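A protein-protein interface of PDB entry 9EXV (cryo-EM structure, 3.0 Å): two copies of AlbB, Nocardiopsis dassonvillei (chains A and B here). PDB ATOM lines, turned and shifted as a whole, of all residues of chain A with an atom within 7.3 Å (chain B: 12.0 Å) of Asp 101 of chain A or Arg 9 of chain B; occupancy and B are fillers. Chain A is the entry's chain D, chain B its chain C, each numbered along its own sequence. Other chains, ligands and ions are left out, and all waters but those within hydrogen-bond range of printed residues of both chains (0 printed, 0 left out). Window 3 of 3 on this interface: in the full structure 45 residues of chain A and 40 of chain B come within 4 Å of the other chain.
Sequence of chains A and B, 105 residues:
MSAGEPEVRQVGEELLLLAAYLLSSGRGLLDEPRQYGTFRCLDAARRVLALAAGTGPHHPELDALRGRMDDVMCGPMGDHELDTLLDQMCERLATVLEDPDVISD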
ATOM      1  N   THR A  55     -19.927  -3.028  -1.877  1.00  0.00           N
ATOM      2  CA  THR A  55     -21.012  -2.050  -1.893  1.00  0.00           C
ATOM      3  C   THR A  55     -20.551  -0.666  -2.334  1.00  0.00           C
ATOM      4  O   THR A  55     -21.298   0.074  -2.983  1.00  0.00           O
ATOM      5  CB  THR A  55     -21.650  -1.958  -0.506  1.00  0.00           C
ATOM      6  OG1 THR A  55     -20.727  -1.354   0.410  1.00  0.00           O
ATOM      7  CG2 THR A  55     -22.030  -3.340   0.001  1.00  0.00           C
ATOM      8  N   GLY A  56     -19.324  -0.305  -1.974  1.00  0.00           N
ATOM      9  CA  GLY A  56     -18.781   1.002  -2.254  1.00  0.00           C
ATOM     10  C   GLY A  56     -18.431   1.259  -3.706  1.00  0.00           C
ATOM     11  O   GLY A  56     -18.775   0.483  -4.605  1.00  0.00           O
ATOM     12  N   PRO A  57     -17.744   2.374  -3.959  1.00  0.00           N
ATOM     13  CA  PRO A  57     -17.424   2.750  -5.341  1.00  0.00           C
ATOM     14  C   PRO A  57     -16.577   1.688  -6.028  1.00  0.00           C
ATOM     15  O   PRO A  57     -15.721   1.051  -5.412  1.00  0.00           O
ATOM     16  CB  PRO A  57     -16.653   4.066  -5.184  1.00  0.00           C
ATOM     17  CG  PRO A  57     -17.013   4.577  -3.828  1.00  0.00           C
ATOM     18  CD  PRO A  57     -17.251   3.363  -2.985  1.00  0.00           C
ATOM     19  N   HIS A  58     -16.830   1.505  -7.321  1.00  0.00           N
ATOM     20  CA  HIS A  58     -16.115   0.536  -8.140  1.00  0.00           C
ATOM     21  C   HIS A  58     -15.091   1.254  -9.007  1.00  0.00           C
ATOM     22  O   HIS A  58     -15.421   2.235  -9.684  1.00  0.00           O
ATOM     23  CB  HIS A  58     -17.082  -0.254  -9.022  1.00  0.00           C
ATOM     24  CG  HIS A  58     -17.656  -1.471  -8.367  1.00  0.00           C
ATOM     25  ND1 HIS A  58     -18.634  -2.239  -8.960  1.00  0.00           N
ATOM     26  CD2 HIS A  58     -17.384  -2.061  -7.179  1.00  0.00           C
ATOM     27  CE1 HIS A  58     -18.944  -3.247  -8.165  1.00  0.00           C
ATOM     28  NE2 HIS A  58     -18.200  -3.162  -7.076  1.00  0.00           N
ATOM     29  N   HIS A  59     -13.853   0.759  -8.994  1.00  0.00           N
ATOM     30  CA  HIS A  59     -12.790   1.293  -9.824  1.00  0.00           C
ATOM     31  C   HIS A  59     -11.892   0.124 -10.204  1.00  0.00           C
ATOM     32  O   HIS A  59     -11.528  -0.668  -9.321  1.00  0.00           O
ATOM     33  CB  HIS A  59     -11.983   2.373  -9.101  1.00  0.00           C
ATOM     34  CG  HIS A  59     -11.083   3.162 -10.000  1.00  0.00           C
ATOM     35  ND1 HIS A  59      -9.808   2.750 -10.326  1.00  0.00           N
ATOM     36  CD2 HIS A  59     -11.269   4.343 -10.636  1.00  0.00           C
ATOM     37  CE1 HIS A  59      -9.251   3.640 -11.127  1.00  0.00           C
ATOM     38  NE2 HIS A  59     -10.116   4.617 -11.330  1.00  0.00           N
ATOM     39  N   VAL A  96      -5.750   6.444  -7.041  1.00  0.00           N
ATOM     40  CA  VAL A  96      -7.161   6.146  -7.257  1.00  0.00           C
ATOM     41  C   VAL A  96      -8.026   7.126  -6.480  1.00  0.00           C
ATOM     42  O   VAL A  96      -8.914   7.767  -7.042  1.00  0.00           O
ATOM     43  CB  VAL A  96      -7.470   4.686  -6.878  1.00  0.00           C
ATOM     44  CG1 VAL A  96      -8.960   4.416  -6.981  1.00  0.00           C
ATOM     45  CG2 VAL A  96      -6.709   3.745  -7.772  1.00  0.00           C
ATOM     46  N   LEU A  97      -7.738   7.294  -5.186  1.00  0.00           N
ATOM     47  CA  LEU A  97      -8.538   8.185  -4.350  1.00  0.00           C
ATOM     48  C   LEU A  97      -8.488   9.625  -4.843  1.00  0.00           C
ATOM     49  O   LEU A  97      -9.442  10.378  -4.649  1.00  0.00           O
ATOM     50  CB  LEU A  97      -8.076   8.108  -2.893  1.00  0.00           C
ATOM     51  CG  LEU A  97      -8.597   6.919  -2.079  1.00  0.00           C
ATOM     52  CD1 LEU A  97      -7.838   5.699  -2.388  1.00  0.00           C
ATOM     53  CD2 LEU A  97      -8.551   7.180  -0.584  1.00  0.00           C
ATOM     54  N   GLU A  98      -7.386  10.025  -5.482  1.00  0.00           N
ATOM     55  CA  GLU A  98      -7.312  11.374  -6.031  1.00  0.00           C
ATOM     56  C   GLU A  98      -8.287  11.573  -7.177  1.00  0.00           C
ATOM     57  O   GLU A  98      -8.608  12.717  -7.512  1.00  0.00           O
ATOM     58  CB  GLU A  98      -5.888  11.692  -6.500  1.00  0.00           C
ATOM     59  CG  GLU A  98      -4.810  11.399  -5.470  1.00  0.00           C
ATOM     60  CD  GLU A  98      -3.570  12.257  -5.639  1.00  0.00           C
ATOM     61  OE1 GLU A  98      -3.653  13.306  -6.310  1.00  0.00           O
ATOM     62  OE2 GLU A  98      -2.512  11.882  -5.092  1.00  0.00           O
ATOM     63  N   ASP A  99      -8.758  10.490  -7.782  1.00  0.00           N
ATOM     64  CA  ASP A  99      -9.782  10.589  -8.807  1.00  0.00           C
ATOM     65  C   ASP A  99     -11.028  11.218  -8.198  1.00  0.00           C
ATOM     66  O   ASP A  99     -11.556  10.690  -7.208  1.00  0.00           O
ATOM     67  CB  ASP A  99     -10.110   9.211  -9.379  1.00  0.00           C
ATOM     68  CG  ASP A  99     -10.997   9.283 -10.602  1.00  0.00           C
ATOM     69  OD1 ASP A  99     -10.621   9.982 -11.566  1.00  0.00           O
ATOM     70  OD2 ASP A  99     -12.066   8.637 -10.606  1.00  0.00           O
ATOM     71  N   PRO A 100     -11.524  12.334  -8.738  1.00  0.00           N
ATOM     72  CA  PRO A 100     -12.715  12.964  -8.151  1.00  0.00           C
ATOM     73  C   PRO A 100     -13.959  12.092  -8.202  1.00  0.00           C
ATOM     74  O   PRO A 100     -14.937  12.405  -7.512  1.00  0.00           O
ATOM     75  CB  PRO A 100     -12.891  14.238  -8.987  1.00  0.00           C
ATOM     76  CG  PRO A 100     -11.527  14.522  -9.528  1.00  0.00           C
ATOM     77  CD  PRO A 100     -10.912  13.177  -9.781  1.00  0.00           C
ATOM     78  N   ASP A 101     -13.959  11.018  -8.991  1.00  0.00           N
ATOM     79  CA  ASP A 101     -15.130  10.159  -9.115  1.00  0.00           C
ATOM     80  C   ASP A 101     -15.167   9.052  -8.067  1.00  0.00           C
ATOM     81  O   ASP A 101     -16.223   8.805  -7.474  1.00  0.00           O
ATOM     82  CB  ASP A 101     -15.187   9.546 -10.516  1.00  0.00           C
ATOM     83  CG  ASP A 101     -16.465   8.768 -10.761  1.00  0.00           C
ATOM     84  OD1 ASP A 101     -17.525   9.406 -10.934  1.00  0.00           O
ATOM     85  OD2 ASP A 101     -16.412   7.521 -10.778  1.00  0.00           O
ATOM     86  N   VAL A 102     -14.043   8.374  -7.824  1.00  0.00           N
ATOM     87  CA  VAL A 102     -14.044   7.275  -6.859  1.00  0.00           C
ATOM     88  C   VAL A 102     -14.394   7.786  -5.468  1.00  0.00           C
ATOM     89  O   VAL A 102     -15.185   7.170  -4.745  1.00  0.00           O
ATOM     90  CB  VAL A 102     -12.689   6.538  -6.866  1.00  0.00           C
ATOM     91  CG1 VAL A 102     -11.603   7.410  -6.295  1.00  0.00           C
ATOM     92  CG2 VAL A 102     -12.781   5.248  -6.067  1.00  0.00           C
ATOM     93  N   ILE A 103     -13.822   8.921  -5.076  1.00  0.00           N
ATOM     94  CA  ILE A 103     -14.045   9.504  -3.766  1.00  0.00           C
ATOM     95  C   ILE A 103     -14.842  10.784  -3.948  1.00  0.00           C
ATOM     96  O   ILE A 103     -14.739  11.470  -4.971  1.00  0.00           O
ATOM     97  CB  ILE A 103     -12.726   9.777  -3.014  1.00  0.00           C
ATOM     98  CG1 ILE A 103     -12.980   9.838  -1.509  1.00  0.00           C
ATOM     99  CG2 ILE A 103     -12.099  11.081  -3.486  1.00  0.00           C
ATOM    100  CD1 ILE A 103     -11.730   9.725  -0.678  1.00  0.00           C
ATOM    101  N   SER A 104     -15.652  11.104  -2.945  1.00  0.00           N
ATOM    102  CA  SER A 104     -16.528  12.261  -2.978  1.00  0.00           C
ATOM    103  C   SER A 104     -16.011  13.327  -2.025  1.00  0.00           C
ATOM    104  O   SER A 104     -15.604  13.025  -0.899  1.00  0.00           O
ATOM    105  CB  SER A 104     -17.960  11.878  -2.605  1.00  0.00           C
ATOM    106  OG  SER A 104     -18.861  12.937  -2.861  1.00  0.00           O
ATOM    107  N   GLU B   7     -26.972   5.931   0.921  1.00  0.00           N
ATOM    108  CA  GLU B   7     -26.139   5.918   2.118  1.00  0.00           C
ATOM    109  C   GLU B   7     -25.037   4.870   1.992  1.00  0.00           C
ATOM    110  O   GLU B   7     -23.963   5.006   2.575  1.00  0.00           O
ATOM    111  CB  GLU B   7     -26.991   5.656   3.361  1.00  0.00           C
ATOM    112  CG  GLU B   7     -26.266   5.891   4.676  1.00  0.00           C
ATOM    113  CD  GLU B   7     -27.192   5.823   5.876  1.00  0.00           C
ATOM    114  OE1 GLU B   7     -28.411   6.029   5.700  1.00  0.00           O
ATOM    115  OE2 GLU B   7     -26.700   5.560   6.993  1.00  0.00           O
ATOM    116  N   VAL B   8     -25.321   3.821   1.217  1.00  0.00           N
ATOM    117  CA  VAL B   8     -24.360   2.737   1.032  1.00  0.00           C
ATOM    118  C   VAL B   8     -23.112   3.238   0.310  1.00  0.00           C
ATOM    119  O   VAL B   8     -21.985   2.865   0.651  1.00  0.00           O
ATOM    120  CB  VAL B   8     -25.033   1.566   0.288  1.00  0.00           C
ATOM    121  CG1 VAL B   8     -25.526   2.000  -1.093  1.00  0.00           C
ATOM    122  CG2 VAL B   8     -24.099   0.387   0.183  1.00  0.00           C
ATOM    123  N   ARG B   9     -23.298   4.103  -0.690  1.00  0.00           N
ATOM    124  CA  ARG B   9     -22.173   4.665  -1.430  1.00  0.00           C
ATOM    125  C   ARG B   9     -21.224   5.421  -0.508  1.00  0.00           C
ATOM    126  O   ARG B   9     -20.000   5.291  -0.615  1.00  0.00           O
ATOM    127  CB  ARG B   9     -22.713   5.583  -2.531  1.00  0.00           C
ATOM    128  CG  ARG B   9     -21.689   6.449  -3.247  1.00  0.00           C
ATOM    129  CD  ARG B   9     -21.109   5.743  -4.456  1.00  0.00           C
ATOM    130  NE  ARG B   9     -20.129   6.575  -5.144  1.00  0.00           N
ATOM    131  CZ  ARG B   9     -19.698   6.359  -6.379  1.00  0.00           C
ATOM    132  NH1 ARG B   9     -20.158   5.355  -7.107  1.00  0.00           N
ATOM    133  NH2 ARG B   9     -18.787   7.176  -6.900  1.00  0.00           N
ATOM    134  N   GLN B  10     -21.774   6.219   0.408  1.00  0.00           N
ATOM    135  CA  GLN B  10     -20.940   6.958   1.349  1.00  0.00           C
ATOM    136  C   GLN B  10     -20.184   6.012   2.274  1.00  0.00           C
ATOM    137  O   GLN B  10     -19.020   6.244   2.603  1.00  0.00           O
ATOM    138  CB  GLN B  10     -21.801   7.940   2.145  1.00  0.00           C
ATOM    139  CG  GLN B  10     -22.245   9.165   1.345  1.00  0.00           C
ATOM    140  CD  GLN B  10     -23.405   8.880   0.406  1.00  0.00           C
ATOM    141  OE1 GLN B  10     -24.241   8.019   0.676  1.00  0.00           O
ATOM    142  NE2 GLN B  10     -23.461   9.607  -0.705  1.00  0.00           N
ATOM    143  N   VAL B  11     -20.832   4.932   2.702  1.00  0.00           N
ATOM    144  CA  VAL B  11     -20.134   3.938   3.510  1.00  0.00           C
ATOM    145  C   VAL B  11     -18.949   3.372   2.739  1.00  0.00           C
ATOM    146  O   VAL B  11     -17.860   3.184   3.292  1.00  0.00           O
ATOM    147  CB  VAL B  11     -21.107   2.831   3.953  1.00  0.00           C
ATOM    148  CG1 VAL B  11     -20.362   1.732   4.688  1.00  0.00           C
ATOM    149  CG2 VAL B  11     -22.200   3.417   4.826  1.00  0.00           C
ATOM    150  N   GLY B  12     -19.139   3.112   1.445  1.00  0.00           N
ATOM    151  CA  GLY B  12     -18.049   2.590   0.641  1.00  0.00           C
ATOM    152  C   GLY B  12     -16.885   3.554   0.505  1.00  0.00           C
ATOM    153  O   GLY B  12     -15.725   3.147   0.586  1.00  0.00           O
ATOM    154  N   GLU B  13     -17.170   4.839   0.274  1.00  0.00           N
ATOM    155  CA  GLU B  13     -16.083   5.805   0.167  1.00  0.00           C
ATOM    156  C   GLU B  13     -15.301   5.893   1.471  1.00  0.00           C
ATOM    157  O   GLU B  13     -14.068   5.931   1.461  1.00  0.00           O
ATOM    158  CB  GLU B  13     -16.623   7.179  -0.240  1.00  0.00           C
ATOM    159  CG  GLU B  13     -17.589   7.773   0.747  1.00  0.00           C
ATOM    160  CD  GLU B  13     -18.172   9.093   0.322  1.00  0.00           C
ATOM    161  OE1 GLU B  13     -17.911   9.509  -0.819  1.00  0.00           O
ATOM    162  OE2 GLU B  13     -18.893   9.713   1.132  1.00  0.00           O
ATOM    163  N   GLU B  14     -15.998   5.905   2.608  1.00  0.00           N
ATOM    164  CA  GLU B  14     -15.297   5.914   3.882  1.00  0.00           C
ATOM    165  C   GLU B  14     -14.486   4.639   4.072  1.00  0.00           C
ATOM    166  O   GLU B  14     -13.406   4.675   4.670  1.00  0.00           O
ATOM    167  CB  GLU B  14     -16.283   6.110   5.035  1.00  0.00           C
ATOM    168  CG  GLU B  14     -17.142   7.357   4.889  1.00  0.00           C
ATOM    169  CD  GLU B  14     -17.781   7.795   6.191  1.00  0.00           C
ATOM    170  OE1 GLU B  14     -17.180   7.564   7.260  1.00  0.00           O
ATOM    171  OE2 GLU B  14     -18.886   8.375   6.144  1.00  0.00           O
ATOM    172  N   LEU B  15     -14.980   3.508   3.562  1.00  0.00           N
ATOM    173  CA  LEU B  15     -14.208   2.271   3.620  1.00  0.00           C
ATOM    174  C   LEU B  15     -12.919   2.384   2.820  1.00  0.00           C
ATOM    175  O   LEU B  15     -11.870   1.887   3.245  1.00  0.00           O
ATOM    176  CB  LEU B  15     -15.045   1.102   3.112  1.00  0.00           C
ATOM    177  CG  LEU B  15     -16.061   0.527   4.095  1.00  0.00           C
ATOM    178  CD1 LEU B  15     -16.975  -0.464   3.397  1.00  0.00           C
ATOM    179  CD2 LEU B  15     -15.346  -0.131   5.262  1.00  0.00           C
ATOM    180  N   LEU B  16     -12.978   3.013   1.644  1.00  0.00           N
ATOM    181  CA  LEU B  16     -11.765   3.212   0.861  1.00  0.00           C
ATOM    182  C   LEU B  16     -10.762   4.068   1.620  1.00  0.00           C
ATOM    183  O   LEU B  16      -9.565   3.767   1.638  1.00  0.00           O
ATOM    184  CB  LEU B  16     -12.104   3.850  -0.485  1.00  0.00           C
ATOM    185  CG  LEU B  16     -13.002   3.017  -1.398  1.00  0.00           C
ATOM    186  CD1 LEU B  16     -13.287   3.757  -2.693  1.00  0.00           C
ATOM    187  CD2 LEU B  16     -12.369   1.663  -1.678  1.00  0.00           C
ATOM    188  N   LEU B  17     -11.232   5.136   2.264  1.00  0.00           N
ATOM    189  CA  LEU B  17     -10.338   5.958   3.067  1.00  0.00           C
ATOM    190  C   LEU B  17      -9.721   5.150   4.200  1.00  0.00           C
ATOM    191  O   LEU B  17      -8.527   5.285   4.489  1.00  0.00           O
ATOM    192  CB  LEU B  17     -11.085   7.173   3.610  1.00  0.00           C
ATOM    193  CG  LEU B  17     -11.362   8.246   2.561  1.00  0.00           C
ATOM    194  CD1 LEU B  17     -12.602   9.043   2.923  1.00  0.00           C
ATOM    195  CD2 LEU B  17     -10.152   9.160   2.413  1.00  0.00           C
ATOM    196  N   LEU B  18     -10.517   4.299   4.849  1.00  0.00           N
ATOM    197  CA  LEU B  18      -9.992   3.478   5.935  1.00  0.00           C
ATOM    198  C   LEU B  18      -8.936   2.503   5.430  1.00  0.00           C
ATOM    199  O   LEU B  18      -7.930   2.262   6.109  1.00  0.00           O
ATOM    200  CB  LEU B  18     -11.134   2.731   6.624  1.00  0.00           C
ATOM    201  CG  LEU B  18     -10.782   1.997   7.919  1.00  0.00           C
ATOM    202  CD1 LEU B  18     -11.991   1.945   8.824  1.00  0.00           C
ATOM    203  CD2 LEU B  18     -10.272   0.589   7.647  1.00  0.00           C
ATOM    204  N   LEU B  51     -17.292   4.012  11.719  1.00  0.00           N
ATOM    205  CA  LEU B  51     -18.052   3.793  10.497  1.00  0.00           C
ATOM    206  C   LEU B  51     -19.323   3.006  10.777  1.00  0.00           C
ATOM    207  O   LEU B  51     -20.384   3.307  10.217  1.00  0.00           O
ATOM    208  CB  LEU B  51     -17.196   3.069   9.458  1.00  0.00           C
ATOM    209  CG  LEU B  51     -15.830   3.690   9.177  1.00  0.00           C
ATOM    210  CD1 LEU B  51     -15.180   3.025   7.978  1.00  0.00           C
ATOM    211  CD2 LEU B  51     -15.948   5.192   8.969  1.00  0.00           C
ATOM    212  N   GLY B  54     -23.146   4.589  12.826  1.00  0.00           N
ATOM    213  CA  GLY B  54     -24.349   5.163  12.255  1.00  0.00           C
ATOM    214  C   GLY B  54     -25.051   4.274  11.250  1.00  0.00           C
ATOM    215  O   GLY B  54     -26.170   4.576  10.827  1.00  0.00           O
ATOM    216  N   THR B  55     -24.412   3.175  10.862  1.00  0.00           N
ATOM    217  CA  THR B  55     -24.962   2.261   9.868  1.00  0.00           C
ATOM    218  C   THR B  55     -25.176   0.854  10.396  1.00  0.00           C
ATOM    219  O   THR B  55     -26.167   0.210  10.040  1.00  0.00           O
ATOM    220  CB  THR B  55     -24.044   2.201   8.639  1.00  0.00           C
ATOM    221  OG1 THR B  55     -22.749   1.726   9.031  1.00  0.00           O
ATOM    222  CG2 THR B  55     -23.908   3.577   8.011  1.00  0.00           C
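Of the printed residues of chain B, Asp 101 of chain A touches Arg 9 (3.1 Å). Of chain A, only Pro 57 and Asp 101 come within 4 Å of Arg 9 of chain B. Gly 56 of chain A touches just one residue of chain B: Gly 12. No residue of chain B comes within 4 Å of Pro 100 of chain A. Of the printed residues of chain B, Val 102 of chain A touches Leu 16 (3.7 Å). Printed residues of chain A within 4 Å of Gly 12 of chain B: Gly 56 (3.4 Å) and Pro 57 (3.5 Å). Printed residues of chain A within 4 Å of Val 8 of chain B: Thr 55 (3.5 Å). Of the printed residues of chain B, Leu 97 of chain A touches Leu 17. Of the printed residues of chain A, Leu 17 of chain B touches Leu 97 (3.9 Å) and Ile 103 (3.5 Å).
Printed residues of chain A that touch a printed residue of chain B: Thr 55, Gly 56, Pro 57, Leu 97, Asp 101, Val 102, Ile 103 and Ser 104. Hydrophobic or aromatic side chains of chain B within 4 Å of the printed part of chain A: Val 8, Leu 16 and Leu 17. Among the printed residues, no Asp or Glu carboxylate lies within 4 Å of a Lys or Arg side-chain nitrogen of the other chain.
Val 8 of chain B touches Thr 55 of chain A (CG2 to CB, 3.5 Å). Gly 12 of chain B touches Gly 56 of chain A. CG of Pro 57 of chain A touches NE of Arg 9 of chain B (3.9 Å). Gly 12 of chain B touches Pro 57 of chain A. N of Glu 13 of chain B touches CD of Pro 57 of chain A, 3.6 Å away. Leu 16 of chain B touches Pro 57 of chain A (CD1 to CG, 3.98 Å). Leu 17 of chain B touches Leu 97 of chain A. Val 102 of chain A touches Leu 16 of chain B. Ile 103 of chain A touches Leu 17 of chain B.
O of Asp 101 of chain A is in hydrogen-bond range of NH2 of Arg 9 of chain B (3.1 Å). The side-chain carboxylate of Glu 13 of chain B lies close to the backbone NH of Ser 104 of chain A (3.5 Å).
The backbone NH (N) of Asp 101 of chain A lies close to the side-chain carboxylate (OD2) of Asp 99 of chain A (3.4 Å). N of Val 102 of chain A is in hydrogen-bond range of OD2 of Asp 99 of chain A, 3.4 Å away.
1 position is printed for both chains. Of the 11 pairs that touch across the chains among the printed residues, none has its exchanged pair printed and touching as well.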
